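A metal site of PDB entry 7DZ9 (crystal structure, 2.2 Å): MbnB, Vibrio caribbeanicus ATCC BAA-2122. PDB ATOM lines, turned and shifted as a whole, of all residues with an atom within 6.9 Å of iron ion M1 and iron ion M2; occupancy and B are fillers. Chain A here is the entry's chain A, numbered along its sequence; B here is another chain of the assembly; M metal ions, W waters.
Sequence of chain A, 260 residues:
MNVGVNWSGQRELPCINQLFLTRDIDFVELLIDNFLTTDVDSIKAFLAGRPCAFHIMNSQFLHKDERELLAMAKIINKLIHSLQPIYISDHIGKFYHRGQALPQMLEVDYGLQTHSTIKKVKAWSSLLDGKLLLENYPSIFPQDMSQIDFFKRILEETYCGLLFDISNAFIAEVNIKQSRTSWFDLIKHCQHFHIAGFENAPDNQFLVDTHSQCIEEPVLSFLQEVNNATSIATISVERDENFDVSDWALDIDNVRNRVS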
ATOM      1  N   GLU A  29     -12.639  29.920 -22.514  1.00  0.00           N
ATOM      2  CA  GLU A  29     -12.630  28.520 -22.099  1.00  0.00           C
ATOM      3  C   GLU A  29     -12.536  27.647 -23.337  1.00  0.00           C
ATOM      4  O   GLU A  29     -13.500  27.522 -24.088  1.00  0.00           O
ATOM      5  CB  GLU A  29     -13.882  28.183 -21.296  1.00  0.00           C
ATOM      6  CG  GLU A  29     -13.757  26.837 -20.579  1.00  0.00           C
ATOM      7  CD  GLU A  29     -15.083  26.346 -20.031  1.00  0.00           C
ATOM      8  OE1 GLU A  29     -15.322  26.499 -18.812  1.00  0.00           O
ATOM      9  OE2 GLU A  29     -15.888  25.804 -20.832  1.00  0.00           O
ATOM     10  N   LEU A  31     -12.599  24.193 -25.235  1.00  0.00           N
ATOM     11  CA  LEU A  31     -12.926  22.766 -25.150  1.00  0.00           C
ATOM     12  C   LEU A  31     -11.670  22.018 -25.588  1.00  0.00           C
ATOM     13  O   LEU A  31     -11.479  21.657 -26.750  1.00  0.00           O
ATOM     14  CB  LEU A  31     -14.148  22.440 -26.002  1.00  0.00           C
ATOM     15  CG  LEU A  31     -14.919  21.174 -25.614  1.00  0.00           C
ATOM     16  CD1 LEU A  31     -15.524  21.305 -24.202  1.00  0.00           C
ATOM     17  CD2 LEU A  31     -16.018  20.851 -26.640  1.00  0.00           C
ATOM     18  N   HIS A  55     -11.839  23.033 -20.648  1.00  0.00           N
ATOM     19  CA  HIS A  55     -13.055  22.255 -20.483  1.00  0.00           C
ATOM     20  C   HIS A  55     -12.918  21.016 -21.363  1.00  0.00           C
ATOM     21  O   HIS A  55     -12.722  21.143 -22.563  1.00  0.00           O
ATOM     22  CB  HIS A  55     -14.259  23.091 -20.904  1.00  0.00           C
ATOM     23  CG  HIS A  55     -15.581  22.562 -20.445  1.00  0.00           C
ATOM     24  ND1 HIS A  55     -15.800  22.090 -19.168  1.00  0.00           N
ATOM     25  CD2 HIS A  55     -16.772  22.503 -21.084  1.00  0.00           C
ATOM     26  CE1 HIS A  55     -17.063  21.715 -19.056  1.00  0.00           C
ATOM     27  NE2 HIS A  55     -17.678  21.960 -20.198  1.00  0.00           N
ATOM     28  N   ILE A  56     -13.070  19.818 -20.774  1.00  0.00           N
ATOM     29  CA  ILE A  56     -12.850  18.559 -21.479  1.00  0.00           C
ATOM     30  C   ILE A  56     -14.204  17.911 -21.742  1.00  0.00           C
ATOM     31  O   ILE A  56     -14.955  17.637 -20.794  1.00  0.00           O
ATOM     32  CB  ILE A  56     -11.936  17.614 -20.699  1.00  0.00           C
ATOM     33  CG1 ILE A  56     -10.612  18.282 -20.365  1.00  0.00           C
ATOM     34  CG2 ILE A  56     -11.729  16.280 -21.448  1.00  0.00           C
ATOM     35  CD1 ILE A  56      -9.939  17.638 -19.161  1.00  0.00           C
ATOM     36  N   MET A  57     -14.523  17.683 -23.006  1.00  0.00           N
ATOM     37  CA  MET A  57     -15.795  17.101 -23.420  1.00  0.00           C
ATOM     38  C   MET A  57     -15.758  15.577 -23.499  1.00  0.00           C
ATOM     39  O   MET A  57     -16.663  14.903 -22.975  1.00  0.00           O
ATOM     40  CB  MET A  57     -16.193  17.683 -24.786  1.00  0.00           C
ATOM     41  CG  MET A  57     -17.246  16.873 -25.513  1.00  0.00           C
ATOM     42  SD  MET A  57     -18.764  16.819 -24.556  1.00  0.00           S
ATOM     43  CE  MET A  57     -18.984  18.525 -24.369  1.00  0.00           C
ATOM     44  N   ASP A  90     -13.986  18.799 -16.462  1.00  0.00           N
ATOM     45  CA  ASP A  90     -14.529  17.710 -17.273  1.00  0.00           C
ATOM     46  C   ASP A  90     -15.994  17.516 -16.875  1.00  0.00           C
ATOM     47  O   ASP A  90     -16.551  18.267 -16.064  1.00  0.00           O
ATOM     48  CB  ASP A  90     -13.702  16.429 -17.084  1.00  0.00           C
ATOM     49  CG  ASP A  90     -13.811  15.439 -18.265  1.00  0.00           C
ATOM     50  OD1 ASP A  90     -14.877  15.344 -18.913  1.00  0.00           O
ATOM     51  OD2 ASP A  90     -12.826  14.715 -18.521  1.00  0.00           O
ATOM     52  N   HIS A  91     -16.624  16.497 -17.456  1.00  0.00           N
ATOM     53  CA  HIS A  91     -18.043  16.225 -17.280  1.00  0.00           C
ATOM     54  C   HIS A  91     -18.263  14.904 -16.567  1.00  0.00           C
ATOM     55  O   HIS A  91     -17.404  14.022 -16.561  1.00  0.00           O
ATOM     56  CB  HIS A  91     -18.756  16.140 -18.635  1.00  0.00           C
ATOM     57  CG  HIS A  91     -18.724  17.418 -19.404  1.00  0.00           C
ATOM     58  ND1 HIS A  91     -17.607  17.844 -20.089  1.00  0.00           N
ATOM     59  CD2 HIS A  91     -19.664  18.379 -19.577  1.00  0.00           C
ATOM     60  CE1 HIS A  91     -17.872  19.006 -20.666  1.00  0.00           C
ATOM     61  NE2 HIS A  91     -19.111  19.347 -20.375  1.00  0.00           N
ATOM     62  N   MET A 105     -24.218  12.867 -25.103  1.00  0.00           N
ATOM     63  CA  MET A 105     -23.808  12.566 -23.736  1.00  0.00           C
ATOM     64  C   MET A 105     -25.051  12.534 -22.850  1.00  0.00           C
ATOM     65  O   MET A 105     -25.740  13.554 -22.719  1.00  0.00           O
ATOM     66  CB  MET A 105     -22.797  13.597 -23.228  1.00  0.00           C
ATOM     67  CG  MET A 105     -22.094  13.245 -21.886  1.00  0.00           C
ATOM     68  SD  MET A 105     -20.957  14.552 -21.249  1.00  0.00           S
ATOM     69  CE  MET A 105     -22.128  15.697 -20.543  1.00  0.00           C
ATOM     70  N   GLU A 135     -18.471  19.375 -13.954  1.00  0.00           N
ATOM     71  CA  GLU A 135     -19.646  20.191 -14.230  1.00  0.00           C
ATOM     72  C   GLU A 135     -20.939  19.427 -13.957  1.00  0.00           C
ATOM     73  O   GLU A 135     -21.065  18.241 -14.289  1.00  0.00           O
ATOM     74  CB  GLU A 135     -19.637  20.672 -15.689  1.00  0.00           C
ATOM     75  CG  GLU A 135     -20.814  21.550 -16.037  1.00  0.00           C
ATOM     76  CD  GLU A 135     -20.805  22.030 -17.496  1.00  0.00           C
ATOM     77  OE1 GLU A 135     -20.003  21.514 -18.283  1.00  0.00           O
ATOM     78  OE2 GLU A 135     -21.632  22.904 -17.834  1.00  0.00           O
ATOM     79  N   ASN A 136     -21.917  20.109 -13.349  1.00  0.00           N
ATOM     80  CA  ASN A 136     -23.251  19.529 -13.153  1.00  0.00           C
ATOM     81  C   ASN A 136     -23.984  19.374 -14.475  1.00  0.00           C
ATOM     82  O   ASN A 136     -23.917  20.233 -15.358  1.00  0.00           O
ATOM     83  CB  ASN A 136     -24.073  20.383 -12.183  1.00  0.00           C
ATOM     84  CG  ASN A 136     -24.139  21.856 -12.587  1.00  0.00           C
ATOM     85  OD1 ASN A 136     -23.110  22.519 -12.728  1.00  0.00           O
ATOM     86  ND2 ASN A 136     -25.362  22.380 -12.753  1.00  0.00           N
ATOM     87  N   LEU A 163     -17.482  22.786 -11.033  1.00  0.00           N
ATOM     88  CA  LEU A 163     -17.745  23.828 -12.015  1.00  0.00           C
ATOM     89  C   LEU A 163     -19.258  23.945 -12.136  1.00  0.00           C
ATOM     90  O   LEU A 163     -19.912  23.036 -12.675  1.00  0.00           O
ATOM     91  CB  LEU A 163     -17.091  23.496 -13.360  1.00  0.00           C
ATOM     92  CG  LEU A 163     -17.383  24.428 -14.558  1.00  0.00           C
ATOM     93  CD1 LEU A 163     -16.819  25.817 -14.332  1.00  0.00           C
ATOM     94  CD2 LEU A 163     -16.821  23.832 -15.854  1.00  0.00           C
ATOM     95  N   PHE A 164     -19.834  25.032 -11.611  1.00  0.00           N
ATOM     96  CA  PHE A 164     -21.277  25.089 -11.468  1.00  0.00           C
ATOM     97  C   PHE A 164     -21.895  25.792 -12.668  1.00  0.00           C
ATOM     98  O   PHE A 164     -21.639  26.979 -12.899  1.00  0.00           O
ATOM     99  CB  PHE A 164     -21.707  25.800 -10.191  1.00  0.00           C
ATOM    100  CG  PHE A 164     -23.190  25.787  -9.968  1.00  0.00           C
ATOM    101  CD1 PHE A 164     -23.876  24.585  -9.723  1.00  0.00           C
ATOM    102  CD2 PHE A 164     -23.911  26.974  -9.998  1.00  0.00           C
ATOM    103  CE1 PHE A 164     -25.242  24.578  -9.502  1.00  0.00           C
ATOM    104  CE2 PHE A 164     -25.289  26.975  -9.780  1.00  0.00           C
ATOM    105  CZ  PHE A 164     -25.953  25.770  -9.524  1.00  0.00           C
ATOM    106  N   ASP A 165     -22.707  25.074 -13.422  1.00  0.00           N
ATOM    107  CA  ASP A 165     -23.396  25.608 -14.573  1.00  0.00           C
ATOM    108  C   ASP A 165     -24.779  26.055 -14.116  1.00  0.00           C
ATOM    109  O   ASP A 165     -25.622  25.233 -13.752  1.00  0.00           O
ATOM    110  CB  ASP A 165     -23.478  24.575 -15.701  1.00  0.00           C
ATOM    111  CG  ASP A 165     -23.952  25.171 -17.031  1.00  0.00           C
ATOM    112  OD1 ASP A 165     -25.026  25.800 -17.060  1.00  0.00           O
ATOM    113  OD2 ASP A 165     -23.268  24.986 -18.062  1.00  0.00           O
ATOM    114  N   ILE A 166     -24.991  27.372 -14.138  1.00  0.00           N
ATOM    115  CA  ILE A 166     -26.202  27.968 -13.588  1.00  0.00           C
ATOM    116  C   ILE A 166     -27.427  27.585 -14.399  1.00  0.00           C
ATOM    117  O   ILE A 166     -28.499  27.298 -13.845  1.00  0.00           O
ATOM    118  CB  ILE A 166     -26.022  29.493 -13.508  1.00  0.00           C
ATOM    119  CG1 ILE A 166     -24.883  29.837 -12.520  1.00  0.00           C
ATOM    120  CG2 ILE A 166     -27.335  30.171 -13.137  1.00  0.00           C
ATOM    121  CD1 ILE A 166     -24.610  31.324 -12.398  1.00  0.00           C
ATOM    122  N   SER A 167     -27.322  27.581 -15.730  1.00  0.00           N
ATOM    123  CA  SER A 167     -28.495  27.247 -16.516  1.00  0.00           C
ATOM    124  C   SER A 167     -28.734  25.737 -16.557  1.00  0.00           C
ATOM    125  O   SER A 167     -29.891  25.317 -16.652  1.00  0.00           O
ATOM    126  CB  SER A 167     -28.398  27.836 -17.934  1.00  0.00           C
ATOM    127  OG  SER A 167     -27.174  27.519 -18.592  1.00  0.00           O
ATOM    128  N   ASN A 168     -27.679  24.905 -16.472  1.00  0.00           N
ATOM    129  CA  ASN A 168     -27.886  23.470 -16.300  1.00  0.00           C
ATOM    130  C   ASN A 168     -28.709  23.170 -15.059  1.00  0.00           C
ATOM    131  O   ASN A 168     -29.603  22.323 -15.084  1.00  0.00           O
ATOM    132  CB  ASN A 168     -26.546  22.736 -16.192  1.00  0.00           C
ATOM    133  CG  ASN A 168     -25.788  22.707 -17.495  1.00  0.00           C
ATOM    134  OD1 ASN A 168     -26.156  23.375 -18.461  1.00  0.00           O
ATOM    135  ND2 ASN A 168     -24.680  21.973 -17.498  1.00  0.00           N
ATOM    136  N   HIS A 194     -20.595  28.577 -15.305  1.00  0.00           N
ATOM    137  CA  HIS A 194     -21.125  28.623 -16.664  1.00  0.00           C
ATOM    138  C   HIS A 194     -22.534  29.209 -16.645  1.00  0.00           C
ATOM    139  O   HIS A 194     -23.296  29.039 -15.689  1.00  0.00           O
ATOM    140  CB  HIS A 194     -21.224  27.215 -17.284  1.00  0.00           C
ATOM    141  CG  HIS A 194     -19.944  26.633 -17.794  1.00  0.00           C
ATOM    142  ND1 HIS A 194     -19.916  25.441 -18.489  1.00  0.00           N
ATOM    143  CD2 HIS A 194     -18.657  27.038 -17.704  1.00  0.00           C
ATOM    144  CE1 HIS A 194     -18.667  25.154 -18.813  1.00  0.00           C
ATOM    145  NE2 HIS A 194     -17.886  26.110 -18.351  1.00  0.00           N
ATOM    146  N   ILE A 195     -22.940  29.819 -17.756  1.00  0.00           N
ATOM    147  CA  ILE A 195     -24.327  30.236 -17.931  1.00  0.00           C
ATOM    148  C   ILE A 195     -24.608  30.309 -19.416  1.00  0.00           C
ATOM    149  O   ILE A 195     -23.736  30.706 -20.205  1.00  0.00           O
ATOM    150  CB  ILE A 195     -24.606  31.570 -17.202  1.00  0.00           C
ATOM    151  CG1 ILE A 195     -26.115  31.790 -16.987  1.00  0.00           C
ATOM    152  CG2 ILE A 195     -23.973  32.761 -17.938  1.00  0.00           C
ATOM    153  CD1 ILE A 195     -26.433  33.102 -16.233  1.00  0.00           C
ATOM    154  N   ALA A 196     -25.810  29.920 -19.811  1.00  0.00           N
ATOM    155  CA  ALA A 196     -26.135  29.806 -21.233  1.00  0.00           C
ATOM    156  C   ALA A 196     -27.649  29.827 -21.437  1.00  0.00           C
ATOM    157  O   ALA A 196     -28.427  29.919 -20.484  1.00  0.00           O
ATOM    158  CB  ALA A 196     -25.545  28.529 -21.836  1.00  0.00           C
ATOM    159  N   ASP A 209     -30.445  21.514 -23.338  1.00  0.00           N
ATOM    160  CA  ASP A 209     -29.295  22.357 -22.987  1.00  0.00           C
ATOM    161  C   ASP A 209     -28.458  22.672 -24.242  1.00  0.00           C
ATOM    162  O   ASP A 209     -27.322  22.231 -24.381  1.00  0.00           O
ATOM    163  CB  ASP A 209     -28.444  21.680 -21.930  1.00  0.00           C
ATOM    164  CG  ASP A 209     -27.297  22.549 -21.460  1.00  0.00           C
ATOM    165  OD1 ASP A 209     -27.468  23.791 -21.423  1.00  0.00           O
ATOM    166  OD2 ASP A 209     -26.219  22.013 -21.159  1.00  0.00           O
ATOM    167  N   HIS A 211     -27.300  25.654 -25.625  1.00  0.00           N
ATOM    168  CA  HIS A 211     -26.376  26.781 -25.741  1.00  0.00           C
ATOM    169  C   HIS A 211     -26.575  27.531 -27.070  1.00  0.00           C
ATOM    170  O   HIS A 211     -25.625  27.900 -27.756  1.00  0.00           O
ATOM    171  CB  HIS A 211     -24.924  26.321 -25.593  1.00  0.00           C
ATOM    172  CG  HIS A 211     -24.648  25.557 -24.336  1.00  0.00           C
ATOM    173  ND1 HIS A 211     -23.504  24.809 -24.137  1.00  0.00           N
ATOM    174  CD2 HIS A 211     -25.383  25.404 -23.198  1.00  0.00           C
ATOM    175  CE1 HIS A 211     -23.534  24.248 -22.948  1.00  0.00           C
ATOM    176  NE2 HIS A 211     -24.666  24.588 -22.357  1.00  0.00           N
ATOM    177  N   SER A 236     -18.267  31.736 -17.661  1.00  0.00           N
ATOM    178  CA  SER A 236     -18.196  31.598 -19.106  1.00  0.00           C
ATOM    179  C   SER A 236     -19.627  31.626 -19.629  1.00  0.00           C
ATOM    180  O   SER A 236     -20.477  30.868 -19.165  1.00  0.00           O
ATOM    181  CB  SER A 236     -17.500  30.287 -19.492  1.00  0.00           C
ATOM    182  OG  SER A 236     -17.724  29.961 -20.844  1.00  0.00           O
ATOM    183  N   GLU A 238     -21.828  30.662 -22.420  1.00  0.00           N
ATOM    184  CA  GLU A 238     -21.617  29.639 -23.441  1.00  0.00           C
ATOM    185  C   GLU A 238     -22.455  29.864 -24.684  1.00  0.00           C
ATOM    186  O   GLU A 238     -23.589  30.328 -24.598  1.00  0.00           O
ATOM    187  CB  GLU A 238     -21.932  28.249 -22.881  1.00  0.00           C
ATOM    188  CG  GLU A 238     -21.301  27.945 -21.541  1.00  0.00           C
ATOM    189  CD  GLU A 238     -21.304  26.458 -21.249  1.00  0.00           C
ATOM    190  OE1 GLU A 238     -22.207  26.009 -20.510  1.00  0.00           O
ATOM    191  OE2 GLU A 238     -20.405  25.743 -21.730  1.00  0.00           O
ATOM    192  N   THR B  17     -19.435  19.565 -29.229  1.00  0.00           N
ATOM    193  CA  THR B  17     -19.779  20.738 -28.428  1.00  0.00           C
ATOM    194  C   THR B  17     -20.536  20.286 -27.195  1.00  0.00           C
ATOM    195  O   THR B  17     -21.098  19.195 -27.158  1.00  0.00           O
ATOM    196  CB  THR B  17     -20.647  21.737 -29.213  1.00  0.00           C
ATOM    197  OG1 THR B  17     -21.865  21.094 -29.597  1.00  0.00           O
ATOM    198  CG2 THR B  17     -19.909  22.261 -30.457  1.00  0.00           C
ATOM    199  N   CYS B  18     -20.580  21.175 -26.196  1.00  0.00           N
ATOM    200  CA  CYS B  18     -21.359  20.871 -25.005  1.00  0.00           C
ATOM    201  C   CYS B  18     -22.849  21.032 -25.242  1.00  0.00           C
ATOM    202  O   CYS B  18     -23.646  20.322 -24.623  1.00  0.00           O
ATOM    203  CB  CYS B  18     -20.955  21.809 -23.862  1.00  0.00           C
ATOM    204  SG  CYS B  18     -19.492  21.351 -22.976  1.00  0.00           S
ATOM    205  N   GLY B  19     -23.224  21.896 -26.181  1.00  0.00           N
ATOM    206  CA  GLY B  19     -24.601  22.080 -26.567  1.00  0.00           C
ATOM    207  C   GLY B  19     -25.246  20.818 -27.074  1.00  0.00           C
ATOM    208  O   GLY B  19     -24.764  20.190 -28.026  1.00  0.00           O
HETATM  209 FE    FE M   1     -21.799  24.269 -19.218  1.00  0.00          FE
HETATM  210 FE    FE M   2     -19.890  21.460 -20.451  1.00  0.00          FE
HETATM  211 FE    FE M   3     -25.237  23.819 -20.444  1.00  0.00          FE
HETATM  212  O   HOH W   1     -23.222  23.032 -19.875  1.00  0.00           O
HETATM  213  O   HOH W   2     -20.410  23.414 -20.632  1.00  0.00           O
HETATM  214  O   HOH W   3     -22.166  20.571 -20.572  1.00  0.00           O
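A ring nitrogen (NE2) of His 194 sits at hydrogen-bond distance from the side-chain carboxylate (OE1) of Glu 29 (2.6 Å).
The side-chain carboxylate of Asp 165 is in hydrogen-bond range of the backbone NH of Asn 168 (2.9 Å).
The backbone NH (N) of Glu 135 is in hydrogen-bond range of the backbone carbonyl oxygen (O) of Asp 90.
The backbone NH (N) of Ile 166 is in hydrogen-bond range of the backbone carbonyl oxygen (O) of His 194 (2.8 Å).
The backbone carbonyl oxygen of Ile 56 is in hydrogen-bond range of a ring nitrogen (ND1) of His 91 (2.8 Å).
The side-chain carboxylate (OD1) of Asp 165 lies within hydrogen-bond range of the side-chain hydroxyl (OG) of Ser 167, at 3.1 Å.
O of Phe 164 lies within hydrogen-bond range of N of His 194 (3.1 Å).
The side-chain amide oxygen (OD1) of Asn 136 lies within hydrogen-bond range of the backbone NH (N) of Asp 165, at 2.7 Å.
Within 4 Å of iron ion M2: His 55, His 91, Glu 135 and Cys 18 of chain B.
Iron ion M2 is bound by water W2 (2.0 Å), OE1 of Glu 135 (2.2 Å), NE2 of His 91 (2.3 Å), NE2 of His 55 (2.3 Å), water W3 (2.4 Å) and SG of Cys 18 of chain B (2.6 Å).
Iron ion M2 has six donor atoms within binding distance.
Iron ion M1 is bound by the side-chain carboxylate (OE2) of Glu 135, water W1, the side-chain carboxylate (OD2) of Asp 165, water W2, the side-chain carboxylate (OE1) of Glu 238 and a ring nitrogen (ND1) of His 194.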
